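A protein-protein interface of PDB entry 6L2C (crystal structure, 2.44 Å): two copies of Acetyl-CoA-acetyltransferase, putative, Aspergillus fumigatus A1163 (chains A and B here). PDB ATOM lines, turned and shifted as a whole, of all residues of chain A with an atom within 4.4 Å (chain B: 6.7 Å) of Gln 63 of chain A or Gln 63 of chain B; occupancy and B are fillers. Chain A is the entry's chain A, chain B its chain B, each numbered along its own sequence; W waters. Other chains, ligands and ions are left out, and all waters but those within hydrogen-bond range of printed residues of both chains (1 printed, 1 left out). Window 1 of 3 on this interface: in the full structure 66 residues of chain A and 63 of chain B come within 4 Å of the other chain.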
ATOM      1  N   ASN A  60      21.693  27.612 -16.804  1.00  0.00           N
ATOM      2  CA  ASN A  60      20.439  27.252 -17.505  1.00  0.00           C
ATOM      3  C   ASN A  60      19.769  26.162 -16.679  1.00  0.00           C
ATOM      4  O   ASN A  60      20.331  25.105 -16.589  1.00  0.00           O
ATOM      5  CB  ASN A  60      20.749  26.765 -18.917  1.00  0.00           C
ATOM      6  CG  ASN A  60      19.559  26.656 -19.837  1.00  0.00           C
ATOM      7  OD1 ASN A  60      19.499  25.776 -20.665  1.00  0.00           O
ATOM      8  ND2 ASN A  60      18.625  27.567 -19.729  1.00  0.00           N
ATOM      9  N   VAL A  61      18.604  26.440 -16.107  1.00  0.00           N
ATOM     10  CA  VAL A  61      17.893  25.475 -15.223  1.00  0.00           C
ATOM     11  C   VAL A  61      17.066  24.475 -16.024  1.00  0.00           C
ATOM     12  O   VAL A  61      17.204  23.290 -15.793  1.00  0.00           O
ATOM     13  CB  VAL A  61      16.983  26.206 -14.232  1.00  0.00           C
ATOM     14  CG1 VAL A  61      16.463  25.258 -13.177  1.00  0.00           C
ATOM     15  CG2 VAL A  61      17.671  27.391 -13.605  1.00  0.00           C
ATOM     16  N   LEU A  62      16.219  24.967 -16.908  1.00  0.00           N
ATOM     17  CA  LEU A  62      15.314  24.100 -17.687  1.00  0.00           C
ATOM     18  C   LEU A  62      15.860  23.958 -19.103  1.00  0.00           C
ATOM     19  O   LEU A  62      15.552  24.762 -19.943  1.00  0.00           O
ATOM     20  CB  LEU A  62      13.915  24.707 -17.605  1.00  0.00           C
ATOM     21  CG  LEU A  62      13.488  25.053 -16.182  1.00  0.00           C
ATOM     22  CD1 LEU A  62      12.217  25.862 -16.151  1.00  0.00           C
ATOM     23  CD2 LEU A  62      13.337  23.808 -15.335  1.00  0.00           C
ATOM     24  N   GLN A  63      16.596  22.877 -19.325  1.00  0.00           N
ATOM     25  CA  GLN A  63      17.306  22.633 -20.595  1.00  0.00           C
ATOM     26  C   GLN A  63      16.524  21.728 -21.541  1.00  0.00           C
ATOM     27  O   GLN A  63      17.081  21.390 -22.556  1.00  0.00           O
ATOM     28  CB  GLN A  63      18.678  22.059 -20.264  1.00  0.00           C
ATOM     29  CG  GLN A  63      19.433  22.888 -19.243  1.00  0.00           C
ATOM     30  CD  GLN A  63      20.634  22.210 -18.652  1.00  0.00           C
ATOM     31  OE1 GLN A  63      21.012  21.135 -19.049  1.00  0.00           O
ATOM     32  NE2 GLN A  63      21.243  22.841 -17.678  1.00  0.00           N
ATOM     33  N   GLY A  64      15.261  21.430 -21.273  1.00  0.00           N
ATOM     34  CA  GLY A  64      14.561  20.506 -22.171  1.00  0.00           C
ATOM     35  C   GLY A  64      14.211  21.211 -23.470  1.00  0.00           C
ATOM     36  O   GLY A  64      13.783  22.376 -23.474  1.00  0.00           O
ATOM     37  N   ALA A  65      14.458  20.539 -24.576  1.00  0.00           N
ATOM     38  CA  ALA A  65      14.120  21.042 -25.913  1.00  0.00           C
ATOM     39  C   ALA A  65      14.953  22.213 -26.367  1.00  0.00           C
ATOM     40  O   ALA A  65      14.718  22.787 -27.432  1.00  0.00           O
ATOM     41  CB  ALA A  65      12.621  21.365 -26.018  1.00  0.00           C
ATOM     42  N   VAL A  66      16.002  22.470 -25.613  1.00  0.00           N
ATOM     43  CA  VAL A  66      16.918  23.588 -25.929  1.00  0.00           C
ATOM     44  C   VAL A  66      17.946  23.107 -26.950  1.00  0.00           C
ATOM     45  O   VAL A  66      18.473  23.919 -27.666  1.00  0.00           O
ATOM     46  CB  VAL A  66      17.566  24.105 -24.640  1.00  0.00           C
ATOM     47  CG1 VAL A  66      18.716  25.043 -24.916  1.00  0.00           C
ATOM     48  CG2 VAL A  66      16.549  24.759 -23.740  1.00  0.00           C
ATOM     49  N   PRO A  70      23.489  23.516 -24.392  1.00  0.00           N
ATOM     50  CA  PRO A  70      22.980  24.882 -24.487  1.00  0.00           C
ATOM     51  C   PRO A  70      24.057  26.000 -24.422  1.00  0.00           C
ATOM     52  O   PRO A  70      24.017  26.948 -25.208  1.00  0.00           O
ATOM     53  CB  PRO A  70      22.064  24.981 -23.277  1.00  0.00           C
ATOM     54  CG  PRO A  70      21.634  23.570 -23.016  1.00  0.00           C
ATOM     55  CD  PRO A  70      22.827  22.747 -23.323  1.00  0.00           C
ATOM     56  N   THR A  88      27.277  23.882 -19.497  1.00  0.00           N
ATOM     57  CA  THR A  88      25.971  24.394 -19.028  1.00  0.00           C
ATOM     58  C   THR A  88      25.901  24.143 -17.522  1.00  0.00           C
ATOM     59  O   THR A  88      26.164  23.055 -17.114  1.00  0.00           O
ATOM     60  CB  THR A  88      24.825  23.822 -19.861  1.00  0.00           C
ATOM     61  OG1 THR A  88      25.224  24.041 -21.203  1.00  0.00           O
ATOM     62  CG2 THR A  88      23.512  24.524 -19.638  1.00  0.00           C
ATOM     63  N   ASN A  90      23.872  24.177 -13.770  1.00  0.00           N
ATOM     64  CA  ASN A  90      22.540  24.095 -13.140  1.00  0.00           C
ATOM     65  C   ASN A  90      22.658  24.092 -11.620  1.00  0.00           C
ATOM     66  O   ASN A  90      22.876  23.051 -11.045  1.00  0.00           O
ATOM     67  CB  ASN A  90      21.716  22.926 -13.668  1.00  0.00           C
ATOM     68  CG  ASN A  90      20.285  22.941 -13.192  1.00  0.00           C
ATOM     69  OD1 ASN A  90      19.831  23.891 -12.593  1.00  0.00           O
ATOM     70  ND2 ASN A  90      19.574  21.868 -13.434  1.00  0.00           N
ATOM     71  N   ASP A 151      10.506  20.646 -12.838  1.00  0.00           N
ATOM     72  CA  ASP A 151      11.972  20.824 -12.712  1.00  0.00           C
ATOM     73  C   ASP A 151      12.375  22.197 -12.162  1.00  0.00           C
ATOM     74  O   ASP A 151      13.501  22.319 -11.716  1.00  0.00           O
ATOM     75  CB  ASP A 151      12.637  20.601 -14.062  1.00  0.00           C
ATOM     76  CG  ASP A 151      12.461  19.202 -14.577  1.00  0.00           C
ATOM     77  OD1 ASP A 151      12.128  18.347 -13.794  1.00  0.00           O
ATOM     78  OD2 ASP A 151      12.668  19.001 -15.743  1.00  0.00           O
ATOM     79  N   MET B  58      27.600  16.539  -9.654  1.00  0.00           N
ATOM     80  CA  MET B  58      27.176  15.380 -10.472  1.00  0.00           C
ATOM     81  C   MET B  58      26.805  15.804 -11.889  1.00  0.00           C
ATOM     82  O   MET B  58      26.084  16.761 -12.057  1.00  0.00           O
ATOM     83  CB  MET B  58      25.978  14.657  -9.853  1.00  0.00           C
ATOM     84  CG  MET B  58      26.260  14.007  -8.524  1.00  0.00           C
ATOM     85  SD  MET B  58      27.268  12.538  -8.574  1.00  0.00           S
ATOM     86  CE  MET B  58      26.051  11.319  -9.040  1.00  0.00           C
ATOM     87  N   GLY B  59      27.348  15.092 -12.861  1.00  0.00           N
ATOM     88  CA  GLY B  59      27.017  15.256 -14.260  1.00  0.00           C
ATOM     89  C   GLY B  59      25.651  14.657 -14.501  1.00  0.00           C
ATOM     90  O   GLY B  59      25.307  13.642 -13.904  1.00  0.00           O
ATOM     91  N   ASN B  60      24.872  15.297 -15.355  1.00  0.00           N
ATOM     92  CA  ASN B  60      23.607  14.761 -15.821  1.00  0.00           C
ATOM     93  C   ASN B  60      23.245  15.451 -17.141  1.00  0.00           C
ATOM     94  O   ASN B  60      23.047  16.670 -17.122  1.00  0.00           O
ATOM     95  CB  ASN B  60      22.553  15.079 -14.754  1.00  0.00           C
ATOM     96  CG  ASN B  60      21.271  14.327 -14.946  1.00  0.00           C
ATOM     97  OD1 ASN B  60      21.244  13.221 -15.487  1.00  0.00           O
ATOM     98  ND2 ASN B  60      20.198  14.898 -14.486  1.00  0.00           N
ATOM     99  N   VAL B  61      23.145  14.746 -18.255  1.00  0.00           N
ATOM    100  CA  VAL B  61      22.934  15.492 -19.526  1.00  0.00           C
ATOM    101  C   VAL B  61      21.468  15.793 -19.835  1.00  0.00           C
ATOM    102  O   VAL B  61      21.203  16.861 -20.317  1.00  0.00           O
ATOM    103  CB  VAL B  61      23.580  14.772 -20.718  1.00  0.00           C
ATOM    104  CG1 VAL B  61      23.407  15.559 -21.993  1.00  0.00           C
ATOM    105  CG2 VAL B  61      25.038  14.475 -20.475  1.00  0.00           C
ATOM    106  N   LEU B  62      20.564  14.890 -19.521  1.00  0.00           N
ATOM    107  CA  LEU B  62      19.165  14.962 -19.936  1.00  0.00           C
ATOM    108  C   LEU B  62      18.326  15.080 -18.673  1.00  0.00           C
ATOM    109  O   LEU B  62      17.989  14.083 -18.016  1.00  0.00           O
ATOM    110  CB  LEU B  62      18.861  13.713 -20.747  1.00  0.00           C
ATOM    111  CG  LEU B  62      19.825  13.586 -21.935  1.00  0.00           C
ATOM    112  CD1 LEU B  62      19.695  12.270 -22.658  1.00  0.00           C
ATOM    113  CD2 LEU B  62      19.602  14.715 -22.916  1.00  0.00           C
ATOM    114  N   GLN B  63      18.061  16.316 -18.296  1.00  0.00           N
ATOM    115  CA  GLN B  63      17.592  16.643 -16.955  1.00  0.00           C
ATOM    116  C   GLN B  63      16.079  16.769 -16.911  1.00  0.00           C
ATOM    117  O   GLN B  63      15.523  17.060 -15.862  1.00  0.00           O
ATOM    118  CB  GLN B  63      18.246  17.928 -16.422  1.00  0.00           C
ATOM    119  CG  GLN B  63      19.746  17.821 -16.247  1.00  0.00           C
ATOM    120  CD  GLN B  63      20.481  19.176 -16.098  1.00  0.00           C
ATOM    121  OE1 GLN B  63      19.894  20.224 -15.790  1.00  0.00           O
ATOM    122  NE2 GLN B  63      21.795  19.141 -16.339  1.00  0.00           N
ATOM    123  N   GLY B  64      15.429  16.548 -18.047  1.00  0.00           N
ATOM    124  CA  GLY B  64      13.980  16.645 -18.139  1.00  0.00           C
ATOM    125  C   GLY B  64      13.266  15.641 -17.259  1.00  0.00           C
ATOM    126  O   GLY B  64      13.535  14.475 -17.328  1.00  0.00           O
ATOM    127  N   ALA B  65      12.382  16.137 -16.415  1.00  0.00           N
ATOM    128  CA  ALA B  65      11.493  15.338 -15.596  1.00  0.00           C
ATOM    129  C   ALA B  65      12.232  14.609 -14.470  1.00  0.00           C
ATOM    130  O   ALA B  65      11.624  13.845 -13.692  1.00  0.00           O
ATOM    131  CB  ALA B  65      10.669  14.383 -16.453  1.00  0.00           C
ATOM    132  N   VAL B  66      13.514  14.923 -14.326  1.00  0.00           N
ATOM    133  CA  VAL B  66      14.286  14.430 -13.208  1.00  0.00           C
ATOM    134  C   VAL B  66      13.892  15.158 -11.928  1.00  0.00           C
ATOM    135  O   VAL B  66      14.214  14.669 -10.856  1.00  0.00           O
ATOM    136  CB  VAL B  66      15.777  14.614 -13.474  1.00  0.00           C
ATOM    137  CG1 VAL B  66      16.615  14.149 -12.302  1.00  0.00           C
ATOM    138  CG2 VAL B  66      16.166  13.818 -14.718  1.00  0.00           C
ATOM    139  N   GLY B  67      13.198  16.300 -12.030  1.00  0.00           N
ATOM    140  CA  GLY B  67      12.884  17.132 -10.862  1.00  0.00           C
ATOM    141  C   GLY B  67      13.941  18.203 -10.561  1.00  0.00           C
ATOM    142  O   GLY B  67      15.020  18.268 -11.178  1.00  0.00           O
ATOM    143  N   PRO B  70      18.956  18.066  -9.873  1.00  0.00           N
ATOM    144  CA  PRO B  70      19.221  16.627  -9.815  1.00  0.00           C
ATOM    145  C   PRO B  70      20.383  16.204  -8.931  1.00  0.00           C
ATOM    146  O   PRO B  70      20.329  15.124  -8.339  1.00  0.00           O
ATOM    147  CB  PRO B  70      19.524  16.267 -11.275  1.00  0.00           C
ATOM    148  CG  PRO B  70      18.722  17.253 -12.070  1.00  0.00           C
ATOM    149  CD  PRO B  70      18.803  18.539 -11.263  1.00  0.00           C
ATOM    150  N   THR B  88      24.512  20.568 -10.631  1.00  0.00           N
ATOM    151  CA  THR B  88      24.421  19.624 -11.732  1.00  0.00           C
ATOM    152  C   THR B  88      25.192  20.178 -12.903  1.00  0.00           C
ATOM    153  O   THR B  88      24.955  21.320 -13.309  1.00  0.00           O
ATOM    154  CB  THR B  88      22.944  19.384 -12.119  1.00  0.00           C
ATOM    155  OG1 THR B  88      22.218  18.994 -10.954  1.00  0.00           O
ATOM    156  CG2 THR B  88      22.825  18.286 -13.108  1.00  0.00           C
ATOM    157  N   VAL B  89      26.146  19.418 -13.421  1.00  0.00           N
ATOM    158  CA  VAL B  89      26.983  19.944 -14.531  1.00  0.00           C
ATOM    159  C   VAL B  89      26.638  19.260 -15.852  1.00  0.00           C
ATOM    160  O   VAL B  89      26.407  18.080 -15.854  1.00  0.00           O
ATOM    161  CB  VAL B  89      28.477  19.923 -14.161  1.00  0.00           C
ATOM    162  CG1 VAL B  89      28.690  19.505 -12.726  1.00  0.00           C
ATOM    163  CG2 VAL B  89      29.336  19.116 -15.099  1.00  0.00           C
ATOM    164  N   ASN B  90      26.586  20.044 -16.924  1.00  0.00           N
ATOM    165  CA  ASN B  90      26.235  19.550 -18.274  1.00  0.00           C
ATOM    166  C   ASN B  90      27.326  19.883 -19.290  1.00  0.00           C
ATOM    167  O   ASN B  90      27.308  20.956 -19.845  1.00  0.00           O
ATOM    168  CB  ASN B  90      24.875  20.072 -18.721  1.00  0.00           C
ATOM    169  CG  ASN B  90      24.349  19.444 -19.990  1.00  0.00           C
ATOM    170  OD1 ASN B  90      25.067  18.803 -20.720  1.00  0.00           O
ATOM    171  ND2 ASN B  90      23.088  19.648 -20.275  1.00  0.00           N
ATOM    172  N   GLU B 121      22.795   9.198 -15.203  1.00  0.00           N
ATOM    173  CA  GLU B 121      21.938   9.276 -16.397  1.00  0.00           C
ATOM    174  C   GLU B 121      20.936   8.134 -16.403  1.00  0.00           C
ATOM    175  O   GLU B 121      21.311   7.030 -16.141  1.00  0.00           O
ATOM    176  CB  GLU B 121      22.777   9.156 -17.662  1.00  0.00           C
ATOM    177  CG  GLU B 121      22.176   9.862 -18.846  1.00  0.00           C
ATOM    178  CD  GLU B 121      22.159  11.367 -18.713  1.00  0.00           C
ATOM    179  OE1 GLU B 121      21.101  11.941 -18.755  1.00  0.00           O
ATOM    180  OE2 GLU B 121      23.202  11.931 -18.561  1.00  0.00           O
ATOM    181  N   VAL B 126      14.243   9.535 -19.979  1.00  0.00           N
ATOM    182  CA  VAL B 126      14.265  10.844 -20.671  1.00  0.00           C
ATOM    183  C   VAL B 126      12.920  10.967 -21.361  1.00  0.00           C
ATOM    184  O   VAL B 126      12.530  10.037 -22.033  1.00  0.00           O
ATOM    185  CB  VAL B 126      15.424  10.961 -21.664  1.00  0.00           C
ATOM    186  CG1 VAL B 126      15.330  12.244 -22.456  1.00  0.00           C
ATOM    187  CG2 VAL B 126      16.760  10.857 -20.971  1.00  0.00           C
ATOM    188  N   PRO B 127      12.203  12.083 -21.205  1.00  0.00           N
ATOM    189  CA  PRO B 127      10.890  12.207 -21.776  1.00  0.00           C
ATOM    190  C   PRO B 127      10.784  12.823 -23.167  1.00  0.00           C
ATOM    191  O   PRO B 127      11.735  13.273 -23.689  1.00  0.00           O
ATOM    192  CB  PRO B 127      10.291  13.235 -20.833  1.00  0.00           C
ATOM    193  CG  PRO B 127      11.429  14.160 -20.567  1.00  0.00           C
ATOM    194  CD  PRO B 127      12.630  13.256 -20.480  1.00  0.00           C
ATOM    195  N   TYR B 129       8.993  15.774 -25.561  1.00  0.00           N
ATOM    196  CA  TYR B 129       8.683  17.176 -25.270  1.00  0.00           C
ATOM    197  C   TYR B 129       7.431  17.638 -26.006  1.00  0.00           C
ATOM    198  O   TYR B 129       7.377  17.613 -27.233  1.00  0.00           O
ATOM    199  CB  TYR B 129       9.864  18.095 -25.640  1.00  0.00           C
ATOM    200  CG  TYR B 129      11.171  17.781 -24.947  1.00  0.00           C
ATOM    201  CD1 TYR B 129      11.227  17.512 -23.579  1.00  0.00           C
ATOM    202  CD2 TYR B 129      12.356  17.800 -25.651  1.00  0.00           C
ATOM    203  CE1 TYR B 129      12.417  17.221 -22.942  1.00  0.00           C
ATOM    204  CE2 TYR B 129      13.559  17.516 -25.046  1.00  0.00           C
ATOM    205  CZ  TYR B 129      13.602  17.241 -23.684  1.00  0.00           C
ATOM    206  OH  TYR B 129      14.827  16.965 -23.083  1.00  0.00           O
ATOM    207  N   ASP B 151      17.972  16.647 -27.395  1.00  0.00           N
ATOM    208  CA  ASP B 151      18.950  17.245 -26.459  1.00  0.00           C
ATOM    209  C   ASP B 151      20.183  16.371 -26.254  1.00  0.00           C
ATOM    210  O   ASP B 151      21.199  16.901 -25.899  1.00  0.00           O
ATOM    211  CB  ASP B 151      18.329  17.467 -25.090  1.00  0.00           C
ATOM    212  CG  ASP B 151      17.205  18.467 -25.074  1.00  0.00           C
ATOM    213  OD1 ASP B 151      17.070  19.188 -26.037  1.00  0.00           O
ATOM    214  OD2 ASP B 151      16.509  18.512 -24.085  1.00  0.00           O
HETATM  215  O   HOH W   1      19.357  18.795 -19.543  1.00  0.00           O
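Water W1 lies within hydrogen-bond range of the backbone carbonyl oxygen of Val 61 of chain B (2.8 Å), the side-chain amide oxygen of Gln 63 of chain A (2.9 Å) and the backbone NH of Gln 63 of chain B (3.1 Å).
O of Asn 60 of chain A is in hydrogen-bond range of NE2 of Gln 63 of chain A, at 2.7 Å. The backbone carbonyl oxygen of Asn 60 of chain B lies within hydrogen-bond range of the side-chain amide nitrogen of Gln 63 of chain B (2.9 Å). The side-chain amide nitrogen of Asn 90 of chain B lies within hydrogen-bond range of the backbone carbonyl oxygen of Val 61 of chain B (3.4 Å). The side-chain hydroxyl of Tyr 129 of chain B is in hydrogen-bond range of the side-chain carboxylate of Asp 151 of chain B.
Gln 63 of chain A touches just these residues of chain B: Gln 63 (3.5 Å), Asn 90 (2.8 Å) and Asp 151 (3.3 Å). Printed residues of chain B within 4 Å of Val 66 of chain A: Asp 151 (3.5 Å). Of the printed residues of chain B, Asp 151 of chain A touches Gln 63, Gly 64, Ala 65, Val 66 and Gly 67. Gly 59 of chain B touches none of the printed residues of chain A. Of chain A, only Gln 63, Asn 90 and Asp 151 come within 4 Å of Gln 63 of chain B. Of the printed residues of chain A, Gly 64 of chain B touches Asp 151 (3.6 Å). Printed residues of chain A within 4 Å of Gly 67 of chain B: Asp 151. Glu 121 of chain B touches none of the printed residues of chain A. Of the printed residues of chain A, Tyr 129 of chain B touches Gly 64 (3.7 Å) and Ala 65 (3.2 Å). The nearest residue of chain B that does not touch Gln 63 of chain A is Val 61 of chain B (4.5 Å). The nearest residue of chain A that does not touch Gln 63 of chain B is Val 61 of chain A (4.1 Å).
The side-chain amide oxygen of Gln 63 of chain A is in hydrogen-bond range of the side-chain amide nitrogen of Gln 63 of chain B, at 3.5 Å. ND2 of Asn 90 of chain B lies within hydrogen-bond range of OE1 of Gln 63 of chain A (2.8 Å). N of Ala 65 of chain A sits at hydrogen-bond distance from OD2 of Asp 151 of chain B (2.9 Å). N of Val 66 of chain A is in hydrogen-bond range of OD1 of Asp 151 of chain B, 3.5 Å away. The backbone carbonyl oxygen (O) of Asn 90 of chain B is in hydrogen-bond range of the backbone NH (N) of Thr 88 of chain A, at 2.9 Å. The side-chain amide oxygen of Gln 63 of chain B is in hydrogen-bond range of the side-chain amide nitrogen of Asn 90 of chain A. O of Asn 90 of chain A sits at hydrogen-bond distance from N of Thr 88 of chain B (3.0 Å). The side-chain carboxylate of Asp 151 of chain A is in hydrogen-bond range of the backbone NH of Ala 65 of chain B (3.0 Å). N of Gly 67 of chain B lies within hydrogen-bond range of OD1 of Asp 151 of chain A, at 2.9 Å. O of Gln 63 of chain A lies close to OD2 of Asp 151 of chain B (3.3 Å). O of Gln 63 of chain B sits close to OD2 of Asp 151 of chain A, 3.5 Å away.
Among the printed residues, pairs that only touch across the chains: Ala 65 of chain A with Tyr 129 of chain B, Gly 64 of chain A with Asp 151 of chain B, Asp 151 of chain A with Gly 64 of chain B, Gly 64 of chain A with Tyr 129 of chain B and Asp 151 of chain A with Val 66 of chain B.
Of the 19 printed residues of chain B, 9 touch a printed residue of chain A. Along chain A the printed residues that touch a printed residue of chain B span positions 63 to 151. Among the printed residues, no Asp or Glu carboxylate lies within 4 Å of a Lys or Arg side-chain nitrogen of the other chain.
Gln 63 of chain A touches its own counterpart, Gln 63 of chain B. Gly 64 of chain A touches Asp 151 of chain B, and with the chains exchanged Asp 151 of chain A touches Gly 64 of chain B. Ala 65 of chain A touches Asp 151 of chain B, and with the chains exchanged Asp 151 of chain A touches Ala 65 of chain B. Val 66 of chain A touches Asp 151 of chain B, and with the chains exchanged Asp 151 of chain A touches Val 66 of chain B. Of the 16 pairs that touch across the chains among the printed residues, 13 have their exchanged pair printed and touching as well.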
